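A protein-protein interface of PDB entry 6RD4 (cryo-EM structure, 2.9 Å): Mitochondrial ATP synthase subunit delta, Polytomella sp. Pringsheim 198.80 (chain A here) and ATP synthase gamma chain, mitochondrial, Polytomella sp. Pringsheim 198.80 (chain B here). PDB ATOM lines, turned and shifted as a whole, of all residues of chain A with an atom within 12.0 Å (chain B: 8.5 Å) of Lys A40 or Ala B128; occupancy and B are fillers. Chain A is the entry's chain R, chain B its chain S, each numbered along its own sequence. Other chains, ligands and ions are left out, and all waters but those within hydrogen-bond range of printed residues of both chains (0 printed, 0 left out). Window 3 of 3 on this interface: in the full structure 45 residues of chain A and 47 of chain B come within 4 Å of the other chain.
The side-chain hydroxyl (OG1) of Thr B126 lies within hydrogen-bond range of the backbone carbonyl oxygen (O) of Thr B123 (3.0 Å).
The backbone carbonyl oxygen (O) of Thr B126 sits at hydrogen-bond distance from the side-chain hydroxyl (OG1) of Thr B130 (3.0 Å).
Of the printed residues of chain A, Ala B128 touches Lys A40.
No residue of chain A comes within 4 Å of Arg B124.
Of chain A, only Trp A37 (2.7 Å) comes within 4 Å of Ala B125.
Thr B126 touches just one residue of chain A: Trp A37 (3.8 Å).
Leu B127 touches none of the printed residues of chain A.
Thr B129 touches just these residues of chain A: Trp A37 and Lys A40.
No residue of chain A comes within 4 Å of Glu B131.
No residue of chain A comes within 4 Å of Ser B132.
Of the printed residues of chain A, Lys B121 touches Leu A45.
Printed residues of chain B within 4 Å of Ile A46: Tyr B122.
Val A47 touches none of the printed residues of chain B.
Arg B157 touches none of the printed residues of chain A.
The nearest residue of chain B that does not touch Lys A40 is Glu B131 (4.1 Å).
The nearest residue of chain A that does not touch Ala B128 is Ala A41 (6.2 Å).
Among the printed residues, pairs that only touch across the chains: Phe A33 with Thr B130, Trp A37 with Tyr B122, Trp A37 with Thr B126, Trp A37 with Thr B129, Lys A40 with Thr B129, Leu A45 with Lys B121 and Leu A45 with Tyr B122.
O of Ala B125 sits at hydrogen-bond distance from NE1 of Trp A37, at 2.7 Å.
O of Ala B128 is in hydrogen-bond range of NZ of Lys A40, at 3.3 Å.
The backbone carbonyl oxygen of Ile A46 is in hydrogen-bond range of the side-chain hydroxyl of Tyr B122, at 2.8 Å.
Of the 17 printed residues of chain A, 5 touch a printed residue of chain B.
Hydrophobic or aromatic side chains of chain A within 4 Å of the printed part of chain B: Phe A33, Trp A37, Leu A45 and Ile A46.
Hydrophobic or aromatic side chains of chain B within 4 Å of the printed part of chain A: Tyr B122, Ala B125 and Ala B128.
Among the printed residues, 10 pairs touch across the chains.
Among the printed residues, no Asp or Glu carboxylate lies within 4 Å of a Lys or Arg side-chain nitrogen of the other chain.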
ATOM      1  N   GLU A  32       1.056 -21.022  23.764  1.00  0.00           N
ATOM      2  CA  GLU A  32       0.405 -21.211  25.051  1.00  0.00           C
ATOM      3  C   GLU A  32      -0.800 -20.303  25.177  1.00  0.00           C
ATOM      4  O   GLU A  32      -1.783 -20.661  25.834  1.00  0.00           O
ATOM      5  CB  GLU A  32       1.409 -20.969  26.180  1.00  0.00           C
ATOM      6  CG  GLU A  32       0.936 -21.183  27.636  1.00  0.00           C
ATOM      7  CD  GLU A  32       0.153 -20.021  28.222  1.00  0.00           C
ATOM      8  OE1 GLU A  32      -0.631 -20.232  29.161  1.00  0.00           O
ATOM      9  OE2 GLU A  32       0.309 -18.894  27.720  1.00  0.00           O
ATOM     10  N   PHE A  33      -0.736 -19.115  24.565  1.00  0.00           N
ATOM     11  CA  PHE A  33      -1.824 -18.155  24.696  1.00  0.00           C
ATOM     12  C   PHE A  33      -3.075 -18.630  23.983  1.00  0.00           C
ATOM     13  O   PHE A  33      -4.172 -18.268  24.394  1.00  0.00           O
ATOM     14  CB  PHE A  33      -1.411 -16.784  24.158  1.00  0.00           C
ATOM     15  CG  PHE A  33      -2.430 -15.687  24.410  1.00  0.00           C
ATOM     16  CD1 PHE A  33      -3.274 -15.254  23.404  1.00  0.00           C
ATOM     17  CD2 PHE A  33      -2.518 -15.076  25.650  1.00  0.00           C
ATOM     18  CE1 PHE A  33      -4.184 -14.244  23.629  1.00  0.00           C
ATOM     19  CE2 PHE A  33      -3.431 -14.067  25.879  1.00  0.00           C
ATOM     20  CZ  PHE A  33      -4.263 -13.654  24.867  1.00  0.00           C
ATOM     21  N   THR A  34      -2.934 -19.455  22.944  1.00  0.00           N
ATOM     22  CA  THR A  34      -4.105 -19.986  22.249  1.00  0.00           C
ATOM     23  C   THR A  34      -4.906 -20.922  23.147  1.00  0.00           C
ATOM     24  O   THR A  34      -6.135 -20.817  23.226  1.00  0.00           O
ATOM     25  CB  THR A  34      -3.684 -20.721  20.973  1.00  0.00           C
ATOM     26  OG1 THR A  34      -3.027 -21.945  21.319  1.00  0.00           O
ATOM     27  CG2 THR A  34      -2.765 -19.869  20.126  1.00  0.00           C
ATOM     28  N   GLU A  35      -4.225 -21.829  23.848  1.00  0.00           N
ATOM     29  CA  GLU A  35      -4.894 -22.859  24.634  1.00  0.00           C
ATOM     30  C   GLU A  35      -5.586 -22.329  25.881  1.00  0.00           C
ATOM     31  O   GLU A  35      -6.615 -22.882  26.279  1.00  0.00           O
ATOM     32  CB  GLU A  35      -3.887 -23.926  25.060  1.00  0.00           C
ATOM     33  CG  GLU A  35      -3.367 -24.797  23.936  1.00  0.00           C
ATOM     34  CD  GLU A  35      -2.083 -25.505  24.313  1.00  0.00           C
ATOM     35  OE1 GLU A  35      -1.391 -26.009  23.407  1.00  0.00           O
ATOM     36  OE2 GLU A  35      -1.753 -25.536  25.516  1.00  0.00           O
ATOM     37  N   VAL A  36      -5.057 -21.277  26.505  1.00  0.00           N
ATOM     38  CA  VAL A  36      -5.679 -20.725  27.703  1.00  0.00           C
ATOM     39  C   VAL A  36      -6.775 -19.730  27.351  1.00  0.00           C
ATOM     40  O   VAL A  36      -7.765 -19.614  28.085  1.00  0.00           O
ATOM     41  CB  VAL A  36      -4.554 -20.138  28.573  1.00  0.00           C
ATOM     42  CG1 VAL A  36      -5.068 -19.273  29.718  1.00  0.00           C
ATOM     43  CG2 VAL A  36      -3.724 -21.276  29.120  1.00  0.00           C
ATOM     44  N   TRP A  37      -6.681 -19.090  26.188  1.00  0.00           N
ATOM     45  CA  TRP A  37      -7.680 -18.101  25.798  1.00  0.00           C
ATOM     46  C   TRP A  37      -8.980 -18.760  25.355  1.00  0.00           C
ATOM     47  O   TRP A  37     -10.026 -18.104  25.320  1.00  0.00           O
ATOM     48  CB  TRP A  37      -7.101 -17.230  24.697  1.00  0.00           C
ATOM     49  CG  TRP A  37      -7.867 -16.078  24.250  1.00  0.00           C
ATOM     50  CD1 TRP A  37      -7.881 -14.843  24.800  1.00  0.00           C
ATOM     51  CD2 TRP A  37      -8.676 -16.014  23.089  1.00  0.00           C
ATOM     52  NE1 TRP A  37      -8.695 -14.010  24.078  1.00  0.00           N
ATOM     53  CE2 TRP A  37      -9.190 -14.710  23.013  1.00  0.00           C
ATOM     54  CE3 TRP A  37      -9.032 -16.940  22.110  1.00  0.00           C
ATOM     55  CZ2 TRP A  37     -10.027 -14.313  22.004  1.00  0.00           C
ATOM     56  CZ3 TRP A  37      -9.869 -16.547  21.128  1.00  0.00           C
ATOM     57  CH2 TRP A  37     -10.351 -15.243  21.070  1.00  0.00           C
ATOM     58  N   ASN A  38      -8.943 -20.053  25.038  1.00  0.00           N
ATOM     59  CA  ASN A  38     -10.161 -20.811  24.795  1.00  0.00           C
ATOM     60  C   ASN A  38     -10.903 -21.156  26.082  1.00  0.00           C
ATOM     61  O   ASN A  38     -11.988 -21.743  26.016  1.00  0.00           O
ATOM     62  CB  ASN A  38      -9.843 -22.093  24.026  1.00  0.00           C
ATOM     63  CG  ASN A  38      -9.125 -21.826  22.718  1.00  0.00           C
ATOM     64  OD1 ASN A  38      -8.244 -22.582  22.316  1.00  0.00           O
ATOM     65  ND2 ASN A  38      -9.487 -20.740  22.057  1.00  0.00           N
ATOM     66  N   LYS A  39     -10.356 -20.804  27.242  1.00  0.00           N
ATOM     67  CA  LYS A  39     -10.996 -21.070  28.520  1.00  0.00           C
ATOM     68  C   LYS A  39     -11.652 -19.844  29.131  1.00  0.00           C
ATOM     69  O   LYS A  39     -12.489 -19.990  30.026  1.00  0.00           O
ATOM     70  CB  LYS A  39      -9.985 -21.644  29.522  1.00  0.00           C
ATOM     71  CG  LYS A  39      -9.851 -23.161  29.501  1.00  0.00           C
ATOM     72  CD  LYS A  39      -9.122 -23.669  28.273  1.00  0.00           C
ATOM     73  CE  LYS A  39      -8.901 -25.157  28.333  1.00  0.00           C
ATOM     74  NZ  LYS A  39      -8.315 -25.662  27.068  1.00  0.00           N
ATOM     75  N   LYS A  40     -11.285 -18.644  28.689  1.00  0.00           N
ATOM     76  CA  LYS A  40     -11.846 -17.429  29.269  1.00  0.00           C
ATOM     77  C   LYS A  40     -12.699 -16.631  28.290  1.00  0.00           C
ATOM     78  O   LYS A  40     -13.673 -15.994  28.698  1.00  0.00           O
ATOM     79  CB  LYS A  40     -10.720 -16.552  29.818  1.00  0.00           C
ATOM     80  CG  LYS A  40     -11.193 -15.493  30.778  1.00  0.00           C
ATOM     81  CD  LYS A  40     -11.848 -16.117  31.996  1.00  0.00           C
ATOM     82  CE  LYS A  40     -10.856 -16.924  32.824  1.00  0.00           C
ATOM     83  NZ  LYS A  40      -9.837 -16.083  33.505  1.00  0.00           N
ATOM     84  N   ALA A  41     -12.348 -16.641  27.012  1.00  0.00           N
ATOM     85  CA  ALA A  41     -13.112 -15.951  25.988  1.00  0.00           C
ATOM     86  C   ALA A  41     -14.328 -16.780  25.588  1.00  0.00           C
ATOM     87  O   ALA A  41     -14.446 -17.945  25.976  1.00  0.00           O
ATOM     88  CB  ALA A  41     -12.225 -15.687  24.774  1.00  0.00           C
ATOM     89  N   PRO A  42     -15.276 -16.194  24.851  1.00  0.00           N
ATOM     90  CA  PRO A  42     -16.273 -17.019  24.163  1.00  0.00           C
ATOM     91  C   PRO A  42     -15.635 -17.945  23.134  1.00  0.00           C
ATOM     92  O   PRO A  42     -14.540 -17.702  22.623  1.00  0.00           O
ATOM     93  CB  PRO A  42     -17.189 -15.987  23.490  1.00  0.00           C
ATOM     94  CG  PRO A  42     -16.493 -14.669  23.650  1.00  0.00           C
ATOM     95  CD  PRO A  42     -15.713 -14.789  24.898  1.00  0.00           C
ATOM     96  N   SER A  43     -16.350 -19.030  22.833  1.00  0.00           N
ATOM     97  CA  SER A  43     -15.889 -19.993  21.841  1.00  0.00           C
ATOM     98  C   SER A  43     -16.157 -19.543  20.415  1.00  0.00           C
ATOM     99  O   SER A  43     -15.703 -20.203  19.475  1.00  0.00           O
ATOM    100  CB  SER A  43     -16.551 -21.355  22.072  1.00  0.00           C
ATOM    101  OG  SER A  43     -16.122 -21.927  23.293  1.00  0.00           O
ATOM    102  N   THR A  44     -16.886 -18.442  20.238  1.00  0.00           N
ATOM    103  CA  THR A  44     -17.104 -17.892  18.909  1.00  0.00           C
ATOM    104  C   THR A  44     -15.824 -17.303  18.333  1.00  0.00           C
ATOM    105  O   THR A  44     -15.548 -17.465  17.139  1.00  0.00           O
ATOM    106  CB  THR A  44     -18.193 -16.824  18.970  1.00  0.00           C
ATOM    107  OG1 THR A  44     -17.794 -15.799  19.888  1.00  0.00           O
ATOM    108  CG2 THR A  44     -19.494 -17.424  19.447  1.00  0.00           C
ATOM    109  N   LEU A  45     -15.035 -16.635  19.166  1.00  0.00           N
ATOM    110  CA  LEU A  45     -13.872 -15.905  18.690  1.00  0.00           C
ATOM    111  C   LEU A  45     -12.679 -16.831  18.490  1.00  0.00           C
ATOM    112  O   LEU A  45     -12.342 -17.630  19.367  1.00  0.00           O
ATOM    113  CB  LEU A  45     -13.519 -14.813  19.690  1.00  0.00           C
ATOM    114  CG  LEU A  45     -14.629 -13.818  19.957  1.00  0.00           C
ATOM    115  CD1 LEU A  45     -14.184 -12.779  20.969  1.00  0.00           C
ATOM    116  CD2 LEU A  45     -15.026 -13.191  18.627  1.00  0.00           C
ATOM    117  N   ILE A  46     -12.036 -16.708  17.350  1.00  0.00           N
ATOM    118  CA  ILE A  46     -10.773 -17.385  17.104  1.00  0.00           C
ATOM    119  C   ILE A  46      -9.679 -16.515  17.688  1.00  0.00           C
ATOM    120  O   ILE A  46      -9.903 -15.336  17.980  1.00  0.00           O
ATOM    121  CB  ILE A  46     -10.537 -17.646  15.607  1.00  0.00           C
ATOM    122  CG1 ILE A  46     -10.690 -16.354  14.813  1.00  0.00           C
ATOM    123  CG2 ILE A  46     -11.505 -18.681  15.103  1.00  0.00           C
ATOM    124  CD1 ILE A  46      -9.885 -16.334  13.542  1.00  0.00           C
ATOM    125  N   VAL A  47      -8.489 -17.093  17.834  1.00  0.00           N
ATOM    126  CA  VAL A  47      -7.402 -16.480  18.608  1.00  0.00           C
ATOM    127  C   VAL A  47      -6.905 -15.233  17.886  1.00  0.00           C
ATOM    128  O   VAL A  47      -6.992 -15.164  16.645  1.00  0.00           O
ATOM    129  CB  VAL A  47      -6.274 -17.501  18.842  1.00  0.00           C
ATOM    130  CG1 VAL A  47      -5.457 -17.789  17.588  1.00  0.00           C
ATOM    131  CG2 VAL A  47      -5.394 -17.125  20.023  1.00  0.00           C
ATOM    132  N   PRO A  48      -6.517 -14.181  18.607  1.00  0.00           N
ATOM    133  CA  PRO A  48      -5.872 -13.052  17.944  1.00  0.00           C
ATOM    134  C   PRO A  48      -4.542 -13.463  17.356  1.00  0.00           C
ATOM    135  O   PRO A  48      -3.899 -14.409  17.812  1.00  0.00           O
ATOM    136  CB  PRO A  48      -5.688 -12.034  19.074  1.00  0.00           C
ATOM    137  CG  PRO A  48      -5.932 -12.777  20.322  1.00  0.00           C
ATOM    138  CD  PRO A  48      -6.908 -13.832  19.978  1.00  0.00           C
ATOM    139  N   LYS B 121     -14.487  -5.903  21.559  1.00  0.00           N
ATOM    140  CA  LYS B 121     -14.821  -7.263  21.952  1.00  0.00           C
ATOM    141  C   LYS B 121     -13.564  -8.091  22.196  1.00  0.00           C
ATOM    142  O   LYS B 121     -13.487  -8.846  23.171  1.00  0.00           O
ATOM    143  CB  LYS B 121     -15.704  -7.871  20.873  1.00  0.00           C
ATOM    144  CG  LYS B 121     -15.946  -9.343  20.963  1.00  0.00           C
ATOM    145  CD  LYS B 121     -16.160  -9.891  19.576  1.00  0.00           C
ATOM    146  CE  LYS B 121     -17.322  -9.220  18.867  1.00  0.00           C
ATOM    147  NZ  LYS B 121     -17.175  -9.264  17.386  1.00  0.00           N
ATOM    148  N   TYR B 122     -12.553  -7.928  21.341  1.00  0.00           N
ATOM    149  CA  TYR B 122     -11.270  -8.591  21.540  1.00  0.00           C
ATOM    150  C   TYR B 122     -10.450  -7.962  22.652  1.00  0.00           C
ATOM    151  O   TYR B 122      -9.423  -8.524  23.041  1.00  0.00           O
ATOM    152  CB  TYR B 122     -10.484  -8.580  20.243  1.00  0.00           C
ATOM    153  CG  TYR B 122     -10.695  -9.795  19.395  1.00  0.00           C
ATOM    154  CD1 TYR B 122     -10.923 -11.024  19.967  1.00  0.00           C
ATOM    155  CD2 TYR B 122     -10.715  -9.705  18.023  1.00  0.00           C
ATOM    156  CE1 TYR B 122     -11.112 -12.139  19.193  1.00  0.00           C
ATOM    157  CE2 TYR B 122     -10.920 -10.814  17.242  1.00  0.00           C
ATOM    158  CZ  TYR B 122     -11.116 -12.027  17.830  1.00  0.00           C
ATOM    159  OH  TYR B 122     -11.318 -13.136  17.048  1.00  0.00           O
ATOM    160  N   THR B 123     -10.860  -6.803  23.164  1.00  0.00           N
ATOM    161  CA  THR B 123     -10.199  -6.250  24.336  1.00  0.00           C
ATOM    162  C   THR B 123     -10.467  -7.105  25.562  1.00  0.00           C
ATOM    163  O   THR B 123      -9.540  -7.670  26.150  1.00  0.00           O
ATOM    164  CB  THR B 123     -10.657  -4.822  24.573  1.00  0.00           C
ATOM    165  OG1 THR B 123     -10.243  -4.012  23.476  1.00  0.00           O
ATOM    166  CG2 THR B 123     -10.047  -4.282  25.837  1.00  0.00           C
ATOM    167  N   ARG B 124     -11.741  -7.248  25.937  1.00  0.00           N
ATOM    168  CA  ARG B 124     -12.119  -8.037  27.104  1.00  0.00           C
ATOM    169  C   ARG B 124     -11.897  -9.527  26.904  1.00  0.00           C
ATOM    170  O   ARG B 124     -11.892 -10.275  27.885  1.00  0.00           O
ATOM    171  CB  ARG B 124     -13.578  -7.773  27.450  1.00  0.00           C
ATOM    172  CG  ARG B 124     -14.509  -7.990  26.280  1.00  0.00           C
ATOM    173  CD  ARG B 124     -15.903  -7.464  26.563  1.00  0.00           C
ATOM    174  NE  ARG B 124     -16.542  -8.173  27.663  1.00  0.00           N
ATOM    175  CZ  ARG B 124     -17.279  -9.266  27.503  1.00  0.00           C
ATOM    176  NH1 ARG B 124     -17.460  -9.764  26.289  1.00  0.00           N
ATOM    177  NH2 ARG B 124     -17.827  -9.864  28.551  1.00  0.00           N
ATOM    178  N   ALA B 125     -11.730  -9.982  25.665  1.00  0.00           N
ATOM    179  CA  ALA B 125     -11.343 -11.366  25.446  1.00  0.00           C
ATOM    180  C   ALA B 125      -9.906 -11.611  25.875  1.00  0.00           C
ATOM    181  O   ALA B 125      -9.569 -12.724  26.282  1.00  0.00           O
ATOM    182  CB  ALA B 125     -11.529 -11.742  23.980  1.00  0.00           C
ATOM    183  N   THR B 126      -9.050 -10.595  25.782  1.00  0.00           N
ATOM    184  CA  THR B 126      -7.700 -10.676  26.318  1.00  0.00           C
ATOM    185  C   THR B 126      -7.562 -10.008  27.678  1.00  0.00           C
ATOM    186  O   THR B 126      -6.583 -10.265  28.385  1.00  0.00           O
ATOM    187  CB  THR B 126      -6.690 -10.048  25.353  1.00  0.00           C
ATOM    188  OG1 THR B 126      -6.792  -8.621  25.412  1.00  0.00           O
ATOM    189  CG2 THR B 126      -6.933 -10.519  23.935  1.00  0.00           C
ATOM    190  N   LEU B 127      -8.496  -9.139  28.053  1.00  0.00           N
ATOM    191  CA  LEU B 127      -8.406  -8.488  29.351  1.00  0.00           C
ATOM    192  C   LEU B 127      -9.050  -9.308  30.463  1.00  0.00           C
ATOM    193  O   LEU B 127      -8.810  -9.039  31.646  1.00  0.00           O
ATOM    194  CB  LEU B 127      -9.024  -7.095  29.277  1.00  0.00           C
ATOM    195  CG  LEU B 127      -8.500  -6.093  30.290  1.00  0.00           C
ATOM    196  CD1 LEU B 127      -7.007  -6.075  30.170  1.00  0.00           C
ATOM    197  CD2 LEU B 127      -9.067  -4.726  29.999  1.00  0.00           C
ATOM    198  N   ALA B 128      -9.852 -10.309  30.122  1.00  0.00           N
ATOM    199  CA  ALA B 128     -10.225 -11.318  31.095  1.00  0.00           C
ATOM    200  C   ALA B 128      -9.289 -12.514  31.074  1.00  0.00           C
ATOM    201  O   ALA B 128      -9.197 -13.231  32.073  1.00  0.00           O
ATOM    202  CB  ALA B 128     -11.661 -11.792  30.858  1.00  0.00           C
ATOM    203  N   THR B 129      -8.575 -12.727  29.970  1.00  0.00           N
ATOM    204  CA  THR B 129      -7.750 -13.923  29.837  1.00  0.00           C
ATOM    205  C   THR B 129      -6.463 -13.811  30.639  1.00  0.00           C
ATOM    206  O   THR B 129      -6.126 -14.707  31.422  1.00  0.00           O
ATOM    207  CB  THR B 129      -7.440 -14.168  28.369  1.00  0.00           C
ATOM    208  OG1 THR B 129      -8.673 -14.370  27.678  1.00  0.00           O
ATOM    209  CG2 THR B 129      -6.560 -15.387  28.201  1.00  0.00           C
ATOM    210  N   THR B 130      -5.744 -12.710  30.475  1.00  0.00           N
ATOM    211  CA  THR B 130      -4.420 -12.568  31.057  1.00  0.00           C
ATOM    212  C   THR B 130      -4.445 -12.207  32.537  1.00  0.00           C
ATOM    213  O   THR B 130      -3.378 -12.155  33.158  1.00  0.00           O
ATOM    214  CB  THR B 130      -3.628 -11.525  30.274  1.00  0.00           C
ATOM    215  OG1 THR B 130      -4.306 -10.264  30.330  1.00  0.00           O
ATOM    216  CG2 THR B 130      -3.506 -11.951  28.828  1.00  0.00           C
ATOM    217  N   GLU B 131      -5.616 -11.957  33.122  1.00  0.00           N
ATOM    218  CA  GLU B 131      -5.707 -11.736  34.565  1.00  0.00           C
ATOM    219  C   GLU B 131      -5.947 -13.076  35.243  1.00  0.00           C
ATOM    220  O   GLU B 131      -7.063 -13.604  35.252  1.00  0.00           O
ATOM    221  CB  GLU B 131      -6.797 -10.736  34.916  1.00  0.00           C
ATOM    222  CG  GLU B 131      -6.479  -9.320  34.503  1.00  0.00           C
ATOM    223  CD  GLU B 131      -7.522  -8.335  34.970  1.00  0.00           C
ATOM    224  OE1 GLU B 131      -8.547  -8.769  35.533  1.00  0.00           O
ATOM    225  OE2 GLU B 131      -7.319  -7.123  34.776  1.00  0.00           O
ATOM    226  N   SER B 132      -4.881 -13.646  35.799  1.00  0.00           N
ATOM    227  CA  SER B 132      -4.991 -14.830  36.637  1.00  0.00           C
ATOM    228  C   SER B 132      -4.736 -14.546  38.111  1.00  0.00           C
ATOM    229  O   SER B 132      -4.839 -15.463  38.929  1.00  0.00           O
ATOM    230  CB  SER B 132      -4.026 -15.911  36.145  1.00  0.00           C
ATOM    231  OG  SER B 132      -3.920 -16.971  37.078  1.00  0.00           O
ATOM    232  N   GLU B 133      -4.414 -13.304  38.475  1.00  0.00           N
ATOM    233  CA  GLU B 133      -4.030 -13.003  39.852  1.00  0.00           C
ATOM    234  C   GLU B 133      -4.585 -11.702  40.404  1.00  0.00           C
ATOM    235  O   GLU B 133      -4.210 -11.339  41.522  1.00  0.00           O
ATOM    236  CB  GLU B 133      -2.500 -12.980  39.992  1.00  0.00           C
ATOM    237  CG  GLU B 133      -1.822 -11.843  39.238  1.00  0.00           C
ATOM    238  CD  GLU B 133      -1.457 -12.212  37.810  1.00  0.00           C
ATOM    239  OE1 GLU B 133      -1.921 -13.260  37.318  1.00  0.00           O
ATOM    240  OE2 GLU B 133      -0.713 -11.443  37.175  1.00  0.00           O
ATOM    241  N   LYS B 135      -4.667  -8.210  38.905  1.00  0.00           N
ATOM    242  CA  LYS B 135      -3.638  -7.220  38.636  1.00  0.00           C
ATOM    243  C   LYS B 135      -4.240  -5.865  38.288  1.00  0.00           C
ATOM    244  O   LYS B 135      -5.420  -5.745  37.954  1.00  0.00           O
ATOM    245  CB  LYS B 135      -2.751  -7.675  37.481  1.00  0.00           C
ATOM    246  CG  LYS B 135      -3.461  -7.697  36.139  1.00  0.00           C
ATOM    247  CD  LYS B 135      -2.459  -7.652  35.001  1.00  0.00           C
ATOM    248  CE  LYS B 135      -3.055  -8.144  33.702  1.00  0.00           C
ATOM    249  NZ  LYS B 135      -2.027  -8.257  32.637  1.00  0.00           N
ATOM    250  N   VAL B 137      -4.748  -2.863  35.758  1.00  0.00           N
ATOM    251  CA  VAL B 137      -4.822  -2.701  34.313  1.00  0.00           C
ATOM    252  C   VAL B 137      -5.259  -1.274  34.028  1.00  0.00           C
ATOM    253  O   VAL B 137      -6.251  -0.803  34.592  1.00  0.00           O
ATOM    254  CB  VAL B 137      -5.787  -3.719  33.674  1.00  0.00           C
ATOM    255  CG1 VAL B 137      -6.297  -3.223  32.366  1.00  0.00           C
ATOM    256  CG2 VAL B 137      -5.096  -5.044  33.459  1.00  0.00           C
ATOM    257  N   ILE B 153     -17.488  -1.310  28.894  1.00  0.00           N
ATOM    258  CA  ILE B 153     -17.032  -2.557  29.499  1.00  0.00           C
ATOM    259  C   ILE B 153     -16.195  -2.270  30.739  1.00  0.00           C
ATOM    260  O   ILE B 153     -16.523  -2.736  31.834  1.00  0.00           O
ATOM    261  CB  ILE B 153     -16.248  -3.417  28.497  1.00  0.00           C
ATOM    262  CG1 ILE B 153     -17.011  -3.567  27.177  1.00  0.00           C
ATOM    263  CG2 ILE B 153     -16.018  -4.781  29.098  1.00  0.00           C
ATOM    264  CD1 ILE B 153     -18.381  -4.192  27.304  1.00  0.00           C
ATOM    265  N   GLU B 154     -15.107  -1.514  30.587  1.00  0.00           N
ATOM    266  CA  GLU B 154     -14.270  -1.112  31.720  1.00  0.00           C
ATOM    267  C   GLU B 154     -14.172   0.407  31.744  1.00  0.00           C
ATOM    268  O   GLU B 154     -13.432   1.001  30.957  1.00  0.00           O
ATOM    269  CB  GLU B 154     -12.876  -1.727  31.653  1.00  0.00           C
ATOM    270  CG  GLU B 154     -12.829  -3.224  31.806  1.00  0.00           C
ATOM    271  CD  GLU B 154     -12.920  -3.940  30.482  1.00  0.00           C
ATOM    272  OE1 GLU B 154     -12.930  -3.261  29.438  1.00  0.00           O
ATOM    273  OE2 GLU B 154     -12.995  -5.186  30.481  1.00  0.00           O
ATOM    274  N   ARG B 157     -11.130   1.241  34.789  1.00  0.00           N
ATOM    275  CA  ARG B 157      -9.745   1.017  34.402  1.00  0.00           C
ATOM    276  C   ARG B 157      -9.367   1.831  33.172  1.00  0.00           C
ATOM    277  O   ARG B 157      -8.203   1.838  32.768  1.00  0.00           O
ATOM    278  CB  ARG B 157      -9.516  -0.470  34.155  1.00  0.00           C
ATOM    279  CG  ARG B 157      -9.904  -1.315  35.340  1.00  0.00           C
ATOM    280  CD  ARG B 157      -9.397  -2.731  35.237  1.00  0.00           C
ATOM    281  NE  ARG B 157     -10.078  -3.511  34.214  1.00  0.00           N
ATOM    282  CZ  ARG B 157      -9.831  -4.797  33.994  1.00  0.00           C
ATOM    283  NH1 ARG B 157     -10.482  -5.462  33.052  1.00  0.00           N
ATOM    284  NH2 ARG B 157      -8.932  -5.420  34.736  1.00  0.00           N
